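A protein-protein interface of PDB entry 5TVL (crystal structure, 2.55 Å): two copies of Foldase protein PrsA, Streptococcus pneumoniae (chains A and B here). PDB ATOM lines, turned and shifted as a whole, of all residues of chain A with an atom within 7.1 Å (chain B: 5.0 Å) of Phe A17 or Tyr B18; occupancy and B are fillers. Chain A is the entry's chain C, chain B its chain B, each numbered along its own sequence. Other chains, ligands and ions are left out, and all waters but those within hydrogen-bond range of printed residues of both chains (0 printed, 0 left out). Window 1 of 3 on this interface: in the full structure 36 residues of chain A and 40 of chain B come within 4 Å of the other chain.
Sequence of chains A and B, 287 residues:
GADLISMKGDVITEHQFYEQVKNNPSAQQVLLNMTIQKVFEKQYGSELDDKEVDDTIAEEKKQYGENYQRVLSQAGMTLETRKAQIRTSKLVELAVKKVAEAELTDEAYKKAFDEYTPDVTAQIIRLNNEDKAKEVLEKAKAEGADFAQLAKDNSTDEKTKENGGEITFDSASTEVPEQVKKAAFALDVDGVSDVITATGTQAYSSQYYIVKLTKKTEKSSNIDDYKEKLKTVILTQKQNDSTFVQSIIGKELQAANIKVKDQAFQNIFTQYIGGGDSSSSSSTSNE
A ring nitrogen (ND1) of His B15 is in hydrogen-bond range of the side-chain carboxylate of Glu A14.
A ring nitrogen (NE2) of His B15 sits at hydrogen-bond distance from the side-chain carboxylate (OE2) of Glu B19.
The side-chain carboxylate of Glu A19 is in hydrogen-bond range of a ring nitrogen (NE2) of His A15, 3.1 Å away.
The side-chain carboxylate (OD2) of Asp B262 lies within hydrogen-bond range of the side-chain hydroxyl (OH) of Tyr B18 (2.7 Å).
The side-chain amide oxygen (OE1) of Gln A16 is in hydrogen-bond range of the backbone NH (N) of Thr A13.
The side-chain amino group (NZ) of Lys B22 is in salt-bridge range of the side-chain carboxylate (OD1) of Asp B262, at 3.4 Å.
The backbone NH (N) of Leu A4 lies within hydrogen-bond range of the backbone carbonyl oxygen (O) of Ile A12 (2.9 Å).
Among the printed residues, pairs that only touch across the chains: Leu A4 with Tyr B18 (3.1 Å), His A15 with Glu B14 (3.2 Å), Tyr A18 with Glu B14 (3.4 Å), Met A34 with Gln B16 (3.5 Å), Phe A17 with Ala B27 (3.5 Å), Glu A14 with Tyr B18 (3.5 Å), Gln A16 with Met B34 (3.5 Å), Ile A12 with Met B34 (3.6 Å), Leu A4 with Asp B262 (3.6 Å), Met A34 with Gln B20 (3.6 Å), Ile A12 with Leu B31 (3.7 Å), Gln A20 with Met B34 (3.7 Å), Val A21 with Ala B27 (3.7 Å), Phe A17 with Tyr B18 (3.7 Å), Phe A17 with Leu B31 (3.7 Å), Tyr A18 with Phe B17 (3.8 Å), Phe A17 with Met B34 (3.9 Å), Met A34 with Phe B17 (3.9 Å), Phe A17 with Phe B265 (3.9 Å) and Leu A4 with Leu B31 (3.997 Å).
Phe A17 touches just these residues of chain B: Tyr B18, Ala B27, Leu B31, Met B34 and Phe B265.
Of the printed residues of chain A, Tyr B18 touches Leu A4, Glu A14 and Phe A17.
Of the printed residues of chain B, Met A34 touches Gln B16, Phe B17 and Gln B20.
Of the printed residues of chain A, Glu B14 touches His A15 (3.2 Å) and Tyr A18 (3.4 Å).
Printed residues of chain B within 4 Å of Tyr A18: Glu B14 and Phe B17.
The nearest residue of chain A that does not touch Tyr B18 is Tyr A18 (5.9 Å).
Of the 15 printed residues of chain B, 11 touch a printed residue of chain A.
Printed residues of chain B that touch a printed residue of chain A: Glu B14, His B15, Gln B16, Phe B17, Tyr B18, Gln B20, Ala B27, Leu B31, Met B34, Asp B262 and Phe B265.
Among the printed residues, 21 pairs touch across the chains.
Gln A16 touches Met B34, and with the chains exchanged Met A34 touches Gln B16.
Phe A17 touches Tyr B18, and with the chains exchanged Tyr A18 touches Phe B17.
Phe A17 touches Met B34, and with the chains exchanged Met A34 touches Phe B17.
Gln A20 touches Met B34, and with the chains exchanged Met A34 touches Gln B20.
10 positions are printed for both chains.
Of the 21 pairs that touch across the chains among the printed residues, 12 have their exchanged pair printed and touching as well.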
ATOM      1  N   ASP A   3     -11.040  18.710  30.974  1.00  0.00           N
ATOM      2  CA  ASP A   3     -12.188  19.627  30.986  1.00  0.00           C
ATOM      3  C   ASP A   3     -11.755  21.040  30.595  1.00  0.00           C
ATOM      4  O   ASP A   3     -10.858  21.607  31.219  1.00  0.00           O
ATOM      5  CB  ASP A   3     -12.836  19.671  32.376  1.00  0.00           C
ATOM      6  CG  ASP A   3     -13.402  18.327  32.813  1.00  0.00           C
ATOM      7  OD1 ASP A   3     -13.730  17.483  31.948  1.00  0.00           O
ATOM      8  OD2 ASP A   3     -13.527  18.121  34.038  1.00  0.00           O
ATOM      9  N   LEU A   4     -12.398  21.598  29.567  1.00  0.00           N
ATOM     10  CA  LEU A   4     -12.128  22.966  29.105  1.00  0.00           C
ATOM     11  C   LEU A   4     -12.976  23.991  29.852  1.00  0.00           C
ATOM     12  O   LEU A   4     -12.471  25.034  30.263  1.00  0.00           O
ATOM     13  CB  LEU A   4     -12.421  23.099  27.608  1.00  0.00           C
ATOM     14  CG  LEU A   4     -11.817  22.065  26.664  1.00  0.00           C
ATOM     15  CD1 LEU A   4     -12.065  22.468  25.217  1.00  0.00           C
ATOM     16  CD2 LEU A   4     -10.332  21.898  26.937  1.00  0.00           C
ATOM     17  N   ILE A  12     -17.785  20.855  29.622  1.00  0.00           N
ATOM     18  CA  ILE A  12     -17.387  20.587  28.241  1.00  0.00           C
ATOM     19  C   ILE A  12     -15.977  20.001  28.306  1.00  0.00           C
ATOM     20  O   ILE A  12     -15.054  20.665  28.784  1.00  0.00           O
ATOM     21  CB  ILE A  12     -17.414  21.861  27.369  1.00  0.00           C
ATOM     22  CG1 ILE A  12     -18.841  22.416  27.317  1.00  0.00           C
ATOM     23  CG2 ILE A  12     -16.905  21.564  25.955  1.00  0.00           C
ATOM     24  CD1 ILE A  12     -18.974  23.740  26.599  1.00  0.00           C
ATOM     25  N   THR A  13     -15.828  18.759  27.839  1.00  0.00           N
ATOM     26  CA  THR A  13     -14.528  18.092  27.780  1.00  0.00           C
ATOM     27  C   THR A  13     -13.798  18.457  26.498  1.00  0.00           C
ATOM     28  O   THR A  13     -14.402  18.938  25.532  1.00  0.00           O
ATOM     29  CB  THR A  13     -14.653  16.552  27.827  1.00  0.00           C
ATOM     30  OG1 THR A  13     -15.309  16.079  26.643  1.00  0.00           O
ATOM     31  CG2 THR A  13     -15.425  16.095  29.063  1.00  0.00           C
ATOM     32  N   GLU A  14     -12.494  18.198  26.502  1.00  0.00           N
ATOM     33  CA  GLU A  14     -11.636  18.415  25.343  1.00  0.00           C
ATOM     34  C   GLU A  14     -12.099  17.595  24.141  1.00  0.00           C
ATOM     35  O   GLU A  14     -12.087  18.099  23.016  1.00  0.00           O
ATOM     36  CB  GLU A  14     -10.187  18.066  25.687  1.00  0.00           C
ATOM     37  CG  GLU A  14      -9.169  18.405  24.609  1.00  0.00           C
ATOM     38  CD  GLU A  14      -7.814  17.774  24.878  1.00  0.00           C
ATOM     39  OE1 GLU A  14      -7.202  18.085  25.923  1.00  0.00           O
ATOM     40  OE2 GLU A  14      -7.360  16.958  24.044  1.00  0.00           O
ATOM     41  N   HIS A  15     -12.493  16.344  24.381  1.00  0.00           N
ATOM     42  CA  HIS A  15     -12.980  15.463  23.316  1.00  0.00           C
ATOM     43  C   HIS A  15     -14.330  15.921  22.749  1.00  0.00           C
ATOM     44  O   HIS A  15     -14.549  15.841  21.539  1.00  0.00           O
ATOM     45  CB  HIS A  15     -13.077  14.019  23.816  1.00  0.00           C
ATOM     46  CG  HIS A  15     -13.608  13.061  22.793  1.00  0.00           C
ATOM     47  ND1 HIS A  15     -14.953  12.787  22.658  1.00  0.00           N
ATOM     48  CD2 HIS A  15     -12.977  12.312  21.857  1.00  0.00           C
ATOM     49  CE1 HIS A  15     -15.127  11.912  21.684  1.00  0.00           C
ATOM     50  NE2 HIS A  15     -13.944  11.608  21.181  1.00  0.00           N
ATOM     51  N   GLN A  16     -15.222  16.393  23.620  1.00  0.00           N
ATOM     52  CA  GLN A  16     -16.504  16.989  23.191  1.00  0.00           C
ATOM     53  C   GLN A  16     -16.264  18.211  22.302  1.00  0.00           C
ATOM     54  O   GLN A  16     -16.919  18.369  21.267  1.00  0.00           O
ATOM     55  CB  GLN A  16     -17.371  17.402  24.393  1.00  0.00           C
ATOM     56  CG  GLN A  16     -18.108  16.253  25.064  1.00  0.00           C
ATOM     57  CD  GLN A  16     -18.813  16.675  26.341  1.00  0.00           C
ATOM     58  OE1 GLN A  16     -18.225  17.313  27.214  1.00  0.00           O
ATOM     59  NE2 GLN A  16     -20.081  16.311  26.456  1.00  0.00           N
ATOM     60  N   PHE A  17     -15.315  19.053  22.713  1.00  0.00           N
ATOM     61  CA  PHE A  17     -14.894  20.189  21.906  1.00  0.00           C
ATOM     62  C   PHE A  17     -14.363  19.752  20.541  1.00  0.00           C
ATOM     63  O   PHE A  17     -14.738  20.340  19.523  1.00  0.00           O
ATOM     64  CB  PHE A  17     -13.838  21.019  22.638  1.00  0.00           C
ATOM     65  CG  PHE A  17     -13.289  22.143  21.817  1.00  0.00           C
ATOM     66  CD1 PHE A  17     -14.116  23.178  21.410  1.00  0.00           C
ATOM     67  CD2 PHE A  17     -11.953  22.163  21.434  1.00  0.00           C
ATOM     68  CE1 PHE A  17     -13.623  24.219  20.643  1.00  0.00           C
ATOM     69  CE2 PHE A  17     -11.452  23.202  20.669  1.00  0.00           C
ATOM     70  CZ  PHE A  17     -12.286  24.232  20.272  1.00  0.00           C
ATOM     71  N   TYR A  18     -13.503  18.728  20.527  1.00  0.00           N
ATOM     72  CA  TYR A  18     -12.961  18.180  19.272  1.00  0.00           C
ATOM     73  C   TYR A  18     -14.064  17.672  18.331  1.00  0.00           C
ATOM     74  O   TYR A  18     -14.033  17.958  17.134  1.00  0.00           O
ATOM     75  CB  TYR A  18     -11.912  17.067  19.515  1.00  0.00           C
ATOM     76  CG  TYR A  18     -11.685  16.188  18.292  1.00  0.00           C
ATOM     77  CD1 TYR A  18     -11.003  16.669  17.172  1.00  0.00           C
ATOM     78  CD2 TYR A  18     -12.203  14.892  18.235  1.00  0.00           C
ATOM     79  CE1 TYR A  18     -10.825  15.876  16.043  1.00  0.00           C
ATOM     80  CE2 TYR A  18     -12.027  14.094  17.113  1.00  0.00           C
ATOM     81  CZ  TYR A  18     -11.342  14.588  16.020  1.00  0.00           C
ATOM     82  OH  TYR A  18     -11.182  13.789  14.917  1.00  0.00           O
ATOM     83  N   GLU A  19     -15.024  16.924  18.874  1.00  0.00           N
ATOM     84  CA  GLU A  19     -16.082  16.317  18.052  1.00  0.00           C
ATOM     85  C   GLU A  19     -16.966  17.355  17.358  1.00  0.00           C
ATOM     86  O   GLU A  19     -17.462  17.097  16.260  1.00  0.00           O
ATOM     87  CB  GLU A  19     -16.942  15.338  18.869  1.00  0.00           C
ATOM     88  CG  GLU A  19     -16.238  14.042  19.288  1.00  0.00           C
ATOM     89  CD  GLU A  19     -15.818  13.149  18.132  1.00  0.00           C
ATOM     90  OE1 GLU A  19     -16.395  13.249  17.026  1.00  0.00           O
ATOM     91  OE2 GLU A  19     -14.892  12.335  18.336  1.00  0.00           O
ATOM     92  N   GLN A  20     -17.152  18.517  17.990  1.00  0.00           N
ATOM     93  CA  GLN A  20     -17.868  19.634  17.367  1.00  0.00           C
ATOM     94  C   GLN A  20     -16.984  20.390  16.374  1.00  0.00           C
ATOM     95  O   GLN A  20     -17.403  20.650  15.243  1.00  0.00           O
ATOM     96  CB  GLN A  20     -18.403  20.608  18.425  1.00  0.00           C
ATOM     97  CG  GLN A  20     -19.515  20.041  19.299  1.00  0.00           C
ATOM     98  CD  GLN A  20     -20.812  19.789  18.547  1.00  0.00           C
ATOM     99  OE1 GLN A  20     -21.343  18.679  18.566  1.00  0.00           O
ATOM    100  NE2 GLN A  20     -21.330  20.821  17.881  1.00  0.00           N
ATOM    101  N   VAL A  21     -15.767  20.731  16.795  1.00  0.00           N
ATOM    102  CA  VAL A  21     -14.880  21.600  16.008  1.00  0.00           C
ATOM    103  C   VAL A  21     -14.253  20.934  14.772  1.00  0.00           C
ATOM    104  O   VAL A  21     -13.780  21.638  13.881  1.00  0.00           O
ATOM    105  CB  VAL A  21     -13.766  22.223  16.902  1.00  0.00           C
ATOM    106  CG1 VAL A  21     -12.612  21.250  17.128  1.00  0.00           C
ATOM    107  CG2 VAL A  21     -13.253  23.536  16.322  1.00  0.00           C
ATOM    108  N   LYS A  22     -14.242  19.600  14.708  1.00  0.00           N
ATOM    109  CA  LYS A  22     -13.597  18.886  13.586  1.00  0.00           C
ATOM    110  C   LYS A  22     -14.216  19.185  12.208  1.00  0.00           C
ATOM    111  O   LYS A  22     -13.522  19.121  11.190  1.00  0.00           O
ATOM    112  CB  LYS A  22     -13.571  17.368  13.830  1.00  0.00           C
ATOM    113  CG  LYS A  22     -14.923  16.666  13.754  1.00  0.00           C
ATOM    114  CD  LYS A  22     -14.777  15.164  13.945  1.00  0.00           C
ATOM    115  CE  LYS A  22     -16.114  14.446  13.831  1.00  0.00           C
ATOM    116  NZ  LYS A  22     -16.001  12.999  14.164  1.00  0.00           N
ATOM    117  N   MET A  34      -0.758  21.242   9.880  1.00  0.00           N
ATOM    118  CA  MET A  34       0.007  20.387  10.800  1.00  0.00           C
ATOM    119  C   MET A  34       0.636  19.186  10.087  1.00  0.00           C
ATOM    120  O   MET A  34       1.805  18.878  10.306  1.00  0.00           O
ATOM    121  CB  MET A  34      -0.877  19.885  11.945  1.00  0.00           C
ATOM    122  CG  MET A  34      -1.142  20.910  13.035  1.00  0.00           C
ATOM    123  SD  MET A  34      -2.282  20.242  14.259  1.00  0.00           S
ATOM    124  CE  MET A  34      -1.147  19.245  15.223  1.00  0.00           C
ATOM    125  N   GLU B  14      -5.117  13.530  18.551  1.00  0.00           N
ATOM    126  CA  GLU B  14      -6.227  14.436  18.825  1.00  0.00           C
ATOM    127  C   GLU B  14      -5.813  15.585  19.747  1.00  0.00           C
ATOM    128  O   GLU B  14      -6.163  16.738  19.492  1.00  0.00           O
ATOM    129  CB  GLU B  14      -7.397  13.660  19.446  1.00  0.00           C
ATOM    130  CG  GLU B  14      -8.677  14.468  19.627  1.00  0.00           C
ATOM    131  CD  GLU B  14      -9.809  13.655  20.227  1.00  0.00           C
ATOM    132  OE1 GLU B  14     -10.106  12.557  19.701  1.00  0.00           O
ATOM    133  OE2 GLU B  14     -10.412  14.123  21.221  1.00  0.00           O
ATOM    134  N   HIS B  15      -5.077  15.263  20.808  1.00  0.00           N
ATOM    135  CA  HIS B  15      -4.641  16.266  21.779  1.00  0.00           C
ATOM    136  C   HIS B  15      -3.661  17.282  21.180  1.00  0.00           C
ATOM    137  O   HIS B  15      -3.712  18.463  21.520  1.00  0.00           O
ATOM    138  CB  HIS B  15      -4.015  15.591  22.995  1.00  0.00           C
ATOM    139  CG  HIS B  15      -3.651  16.545  24.088  1.00  0.00           C
ATOM    140  ND1 HIS B  15      -4.526  16.890  25.095  1.00  0.00           N
ATOM    141  CD2 HIS B  15      -2.510  17.233  24.328  1.00  0.00           C
ATOM    142  CE1 HIS B  15      -3.938  17.743  25.914  1.00  0.00           C
ATOM    143  NE2 HIS B  15      -2.714  17.967  25.470  1.00  0.00           N
ATOM    144  N   GLN B  16      -2.779  16.818  20.296  1.00  0.00           N
ATOM    145  CA  GLN B  16      -1.873  17.711  19.553  1.00  0.00           C
ATOM    146  C   GLN B  16      -2.629  18.644  18.614  1.00  0.00           C
ATOM    147  O   GLN B  16      -2.261  19.807  18.456  1.00  0.00           O
ATOM    148  CB  GLN B  16      -0.878  16.904  18.728  1.00  0.00           C
ATOM    149  CG  GLN B  16       0.159  16.175  19.562  1.00  0.00           C
ATOM    150  CD  GLN B  16       0.909  15.118  18.777  1.00  0.00           C
ATOM    151  OE1 GLN B  16       0.472  14.682  17.708  1.00  0.00           O
ATOM    152  NE2 GLN B  16       2.049  14.695  19.310  1.00  0.00           N
ATOM    153  N   PHE B  17      -3.667  18.106  17.976  1.00  0.00           N
ATOM    154  CA  PHE B  17      -4.574  18.902  17.166  1.00  0.00           C
ATOM    155  C   PHE B  17      -5.351  19.908  18.020  1.00  0.00           C
ATOM    156  O   PHE B  17      -5.494  21.068  17.616  1.00  0.00           O
ATOM    157  CB  PHE B  17      -5.541  18.013  16.380  1.00  0.00           C
ATOM    158  CG  PHE B  17      -6.626  18.780  15.673  1.00  0.00           C
ATOM    159  CD1 PHE B  17      -6.303  19.718  14.702  1.00  0.00           C
ATOM    160  CD2 PHE B  17      -7.968  18.574  15.985  1.00  0.00           C
ATOM    161  CE1 PHE B  17      -7.288  20.428  14.049  1.00  0.00           C
ATOM    162  CE2 PHE B  17      -8.965  19.279  15.329  1.00  0.00           C
ATOM    163  CZ  PHE B  17      -8.624  20.209  14.359  1.00  0.00           C
ATOM    164  N   TYR B  18      -5.844  19.469  19.183  1.00  0.00           N
ATOM    165  CA  TYR B  18      -6.498  20.381  20.130  1.00  0.00           C
ATOM    166  C   TYR B  18      -5.578  21.540  20.524  1.00  0.00           C
ATOM    167  O   TYR B  18      -6.008  22.698  20.512  1.00  0.00           O
ATOM    168  CB  TYR B  18      -7.004  19.672  21.400  1.00  0.00           C
ATOM    169  CG  TYR B  18      -7.333  20.668  22.500  1.00  0.00           C
ATOM    170  CD1 TYR B  18      -8.429  21.529  22.383  1.00  0.00           C
ATOM    171  CD2 TYR B  18      -6.512  20.799  23.623  1.00  0.00           C
ATOM    172  CE1 TYR B  18      -8.710  22.471  23.367  1.00  0.00           C
ATOM    173  CE2 TYR B  18      -6.788  21.732  24.612  1.00  0.00           C
ATOM    174  CZ  TYR B  18      -7.883  22.568  24.482  1.00  0.00           C
ATOM    175  OH  TYR B  18      -8.151  23.492  25.466  1.00  0.00           O
ATOM    176  N   GLU B  19      -4.327  21.230  20.869  1.00  0.00           N
ATOM    177  CA  GLU B  19      -3.374  22.260  21.304  1.00  0.00           C
ATOM    178  C   GLU B  19      -3.064  23.310  20.234  1.00  0.00           C
ATOM    179  O   GLU B  19      -2.778  24.458  20.574  1.00  0.00           O
ATOM    180  CB  GLU B  19      -2.063  21.638  21.819  1.00  0.00           C
ATOM    181  CG  GLU B  19      -2.155  20.933  23.175  1.00  0.00           C
ATOM    182  CD  GLU B  19      -2.741  21.798  24.278  1.00  0.00           C
ATOM    183  OE1 GLU B  19      -2.425  23.008  24.316  1.00  0.00           O
ATOM    184  OE2 GLU B  19      -3.527  21.266  25.098  1.00  0.00           O
ATOM    185  N   GLN B  20      -3.119  22.924  18.958  1.00  0.00           N
ATOM    186  CA  GLN B  20      -2.951  23.876  17.847  1.00  0.00           C
ATOM    187  C   GLN B  20      -4.239  24.638  17.538  1.00  0.00           C
ATOM    188  O   GLN B  20      -4.208  25.856  17.344  1.00  0.00           O
ATOM    189  CB  GLN B  20      -2.447  23.171  16.580  1.00  0.00           C
ATOM    190  CG  GLN B  20      -1.017  22.660  16.675  1.00  0.00           C
ATOM    191  CD  GLN B  20      -0.004  23.774  16.862  1.00  0.00           C
ATOM    192  OE1 GLN B  20       0.721  23.799  17.854  1.00  0.00           O
ATOM    193  NE2 GLN B  20       0.041  24.712  15.919  1.00  0.00           N
ATOM    194  N   VAL B  21      -5.364  23.925  17.504  1.00  0.00           N
ATOM    195  CA  VAL B  21      -6.642  24.509  17.088  1.00  0.00           C
ATOM    196  C   VAL B  21      -7.306  25.403  18.148  1.00  0.00           C
ATOM    197  O   VAL B  21      -8.119  26.253  17.792  1.00  0.00           O
ATOM    198  CB  VAL B  21      -7.628  23.414  16.603  1.00  0.00           C
ATOM    199  CG1 VAL B  21      -8.301  22.700  17.770  1.00  0.00           C
ATOM    200  CG2 VAL B  21      -8.666  23.997  15.653  1.00  0.00           C
ATOM    201  N   LYS B  22      -6.962  25.234  19.428  1.00  0.00           N
ATOM    202  CA  LYS B  22      -7.567  26.042  20.507  1.00  0.00           C
ATOM    203  C   LYS B  22      -7.376  27.565  20.358  1.00  0.00           C
ATOM    204  O   LYS B  22      -8.206  28.343  20.839  1.00  0.00           O
ATOM    205  CB  LYS B  22      -7.077  25.582  21.890  1.00  0.00           C
ATOM    206  CG  LYS B  22      -5.621  25.898  22.210  1.00  0.00           C
ATOM    207  CD  LYS B  22      -5.234  25.386  23.589  1.00  0.00           C
ATOM    208  CE  LYS B  22      -3.836  25.847  23.977  1.00  0.00           C
ATOM    209  NZ  LYS B  22      -3.504  25.490  25.385  1.00  0.00           N
ATOM    210  N   ALA B  27     -12.517  28.463  15.946  1.00  0.00           N
ATOM    211  CA  ALA B  27     -12.645  27.397  16.944  1.00  0.00           C
ATOM    212  C   ALA B  27     -13.075  27.933  18.312  1.00  0.00           C
ATOM    213  O   ALA B  27     -13.893  27.310  18.983  1.00  0.00           O
ATOM    214  CB  ALA B  27     -11.342  26.619  17.072  1.00  0.00           C
ATOM    215  N   VAL B  30     -16.711  28.279  18.505  1.00  0.00           N
ATOM    216  CA  VAL B  30     -17.409  26.991  18.645  1.00  0.00           C
ATOM    217  C   VAL B  30     -17.586  26.609  20.115  1.00  0.00           C
ATOM    218  O   VAL B  30     -18.682  26.209  20.509  1.00  0.00           O
ATOM    219  CB  VAL B  30     -16.704  25.855  17.858  1.00  0.00           C
ATOM    220  CG1 VAL B  30     -17.285  24.486  18.197  1.00  0.00           C
ATOM    221  CG2 VAL B  30     -16.818  26.100  16.359  1.00  0.00           C
ATOM    222  N   LEU B  31     -16.527  26.744  20.916  1.00  0.00           N
ATOM    223  CA  LEU B  31     -16.614  26.468  22.356  1.00  0.00           C
ATOM    224  C   LEU B  31     -17.582  27.410  23.068  1.00  0.00           C
ATOM    225  O   LEU B  31     -18.334  26.975  23.942  1.00  0.00           O
ATOM    226  CB  LEU B  31     -15.248  26.565  23.041  1.00  0.00           C
ATOM    227  CG  LEU B  31     -15.245  26.125  24.514  1.00  0.00           C
ATOM    228  CD1 LEU B  31     -15.385  24.614  24.627  1.00  0.00           C
ATOM    229  CD2 LEU B  31     -13.988  26.597  25.216  1.00  0.00           C
ATOM    230  N   MET B  34     -20.970  26.235  22.218  1.00  0.00           N
ATOM    231  CA  MET B  34     -21.242  25.013  22.987  1.00  0.00           C
ATOM    232  C   MET B  34     -21.651  25.335  24.425  1.00  0.00           C
ATOM    233  O   MET B  34     -22.558  24.702  24.969  1.00  0.00           O
ATOM    234  CB  MET B  34     -20.027  24.075  23.013  1.00  0.00           C
ATOM    235  CG  MET B  34     -19.780  23.290  21.740  1.00  0.00           C
ATOM    236  SD  MET B  34     -18.201  22.416  21.815  1.00  0.00           S
ATOM    237  CE  MET B  34     -18.641  21.023  22.860  1.00  0.00           C
ATOM    238  N   ASP B 262      -9.044  26.184  30.477  1.00  0.00           N
ATOM    239  CA  ASP B 262      -7.920  26.432  29.566  1.00  0.00           C
ATOM    240  C   ASP B 262      -7.793  27.929  29.309  1.00  0.00           C
ATOM    241  O   ASP B 262      -8.735  28.563  28.836  1.00  0.00           O
ATOM    242  CB  ASP B 262      -8.113  25.681  28.239  1.00  0.00           C
ATOM    243  CG  ASP B 262      -6.820  25.562  27.427  1.00  0.00           C
ATOM    244  OD1 ASP B 262      -6.290  26.592  26.960  1.00  0.00           O
ATOM    245  OD2 ASP B 262      -6.346  24.424  27.235  1.00  0.00           O
ATOM    246  N   PHE B 265      -8.985  30.148  25.957  1.00  0.00           N
ATOM    247  CA  PHE B 265     -10.353  30.663  25.762  1.00  0.00           C
ATOM    248  C   PHE B 265     -10.762  31.795  26.711  1.00  0.00           C
ATOM    249  O   PHE B 265     -11.882  32.286  26.620  1.00  0.00           O
ATOM    250  CB  PHE B 265     -11.365  29.524  25.904  1.00  0.00           C
ATOM    251  CG  PHE B 265     -11.124  28.385  24.963  1.00  0.00           C
ATOM    252  CD1 PHE B 265     -11.438  28.506  23.614  1.00  0.00           C
ATOM    253  CD2 PHE B 265     -10.590  27.191  25.422  1.00  0.00           C
ATOM    254  CE1 PHE B 265     -11.219  27.454  22.737  1.00  0.00           C
ATOM    255  CE2 PHE B 265     -10.367  26.136  24.553  1.00  0.00           C
ATOM    256  CZ  PHE B 265     -10.682  26.267  23.208  1.00  0.00           C
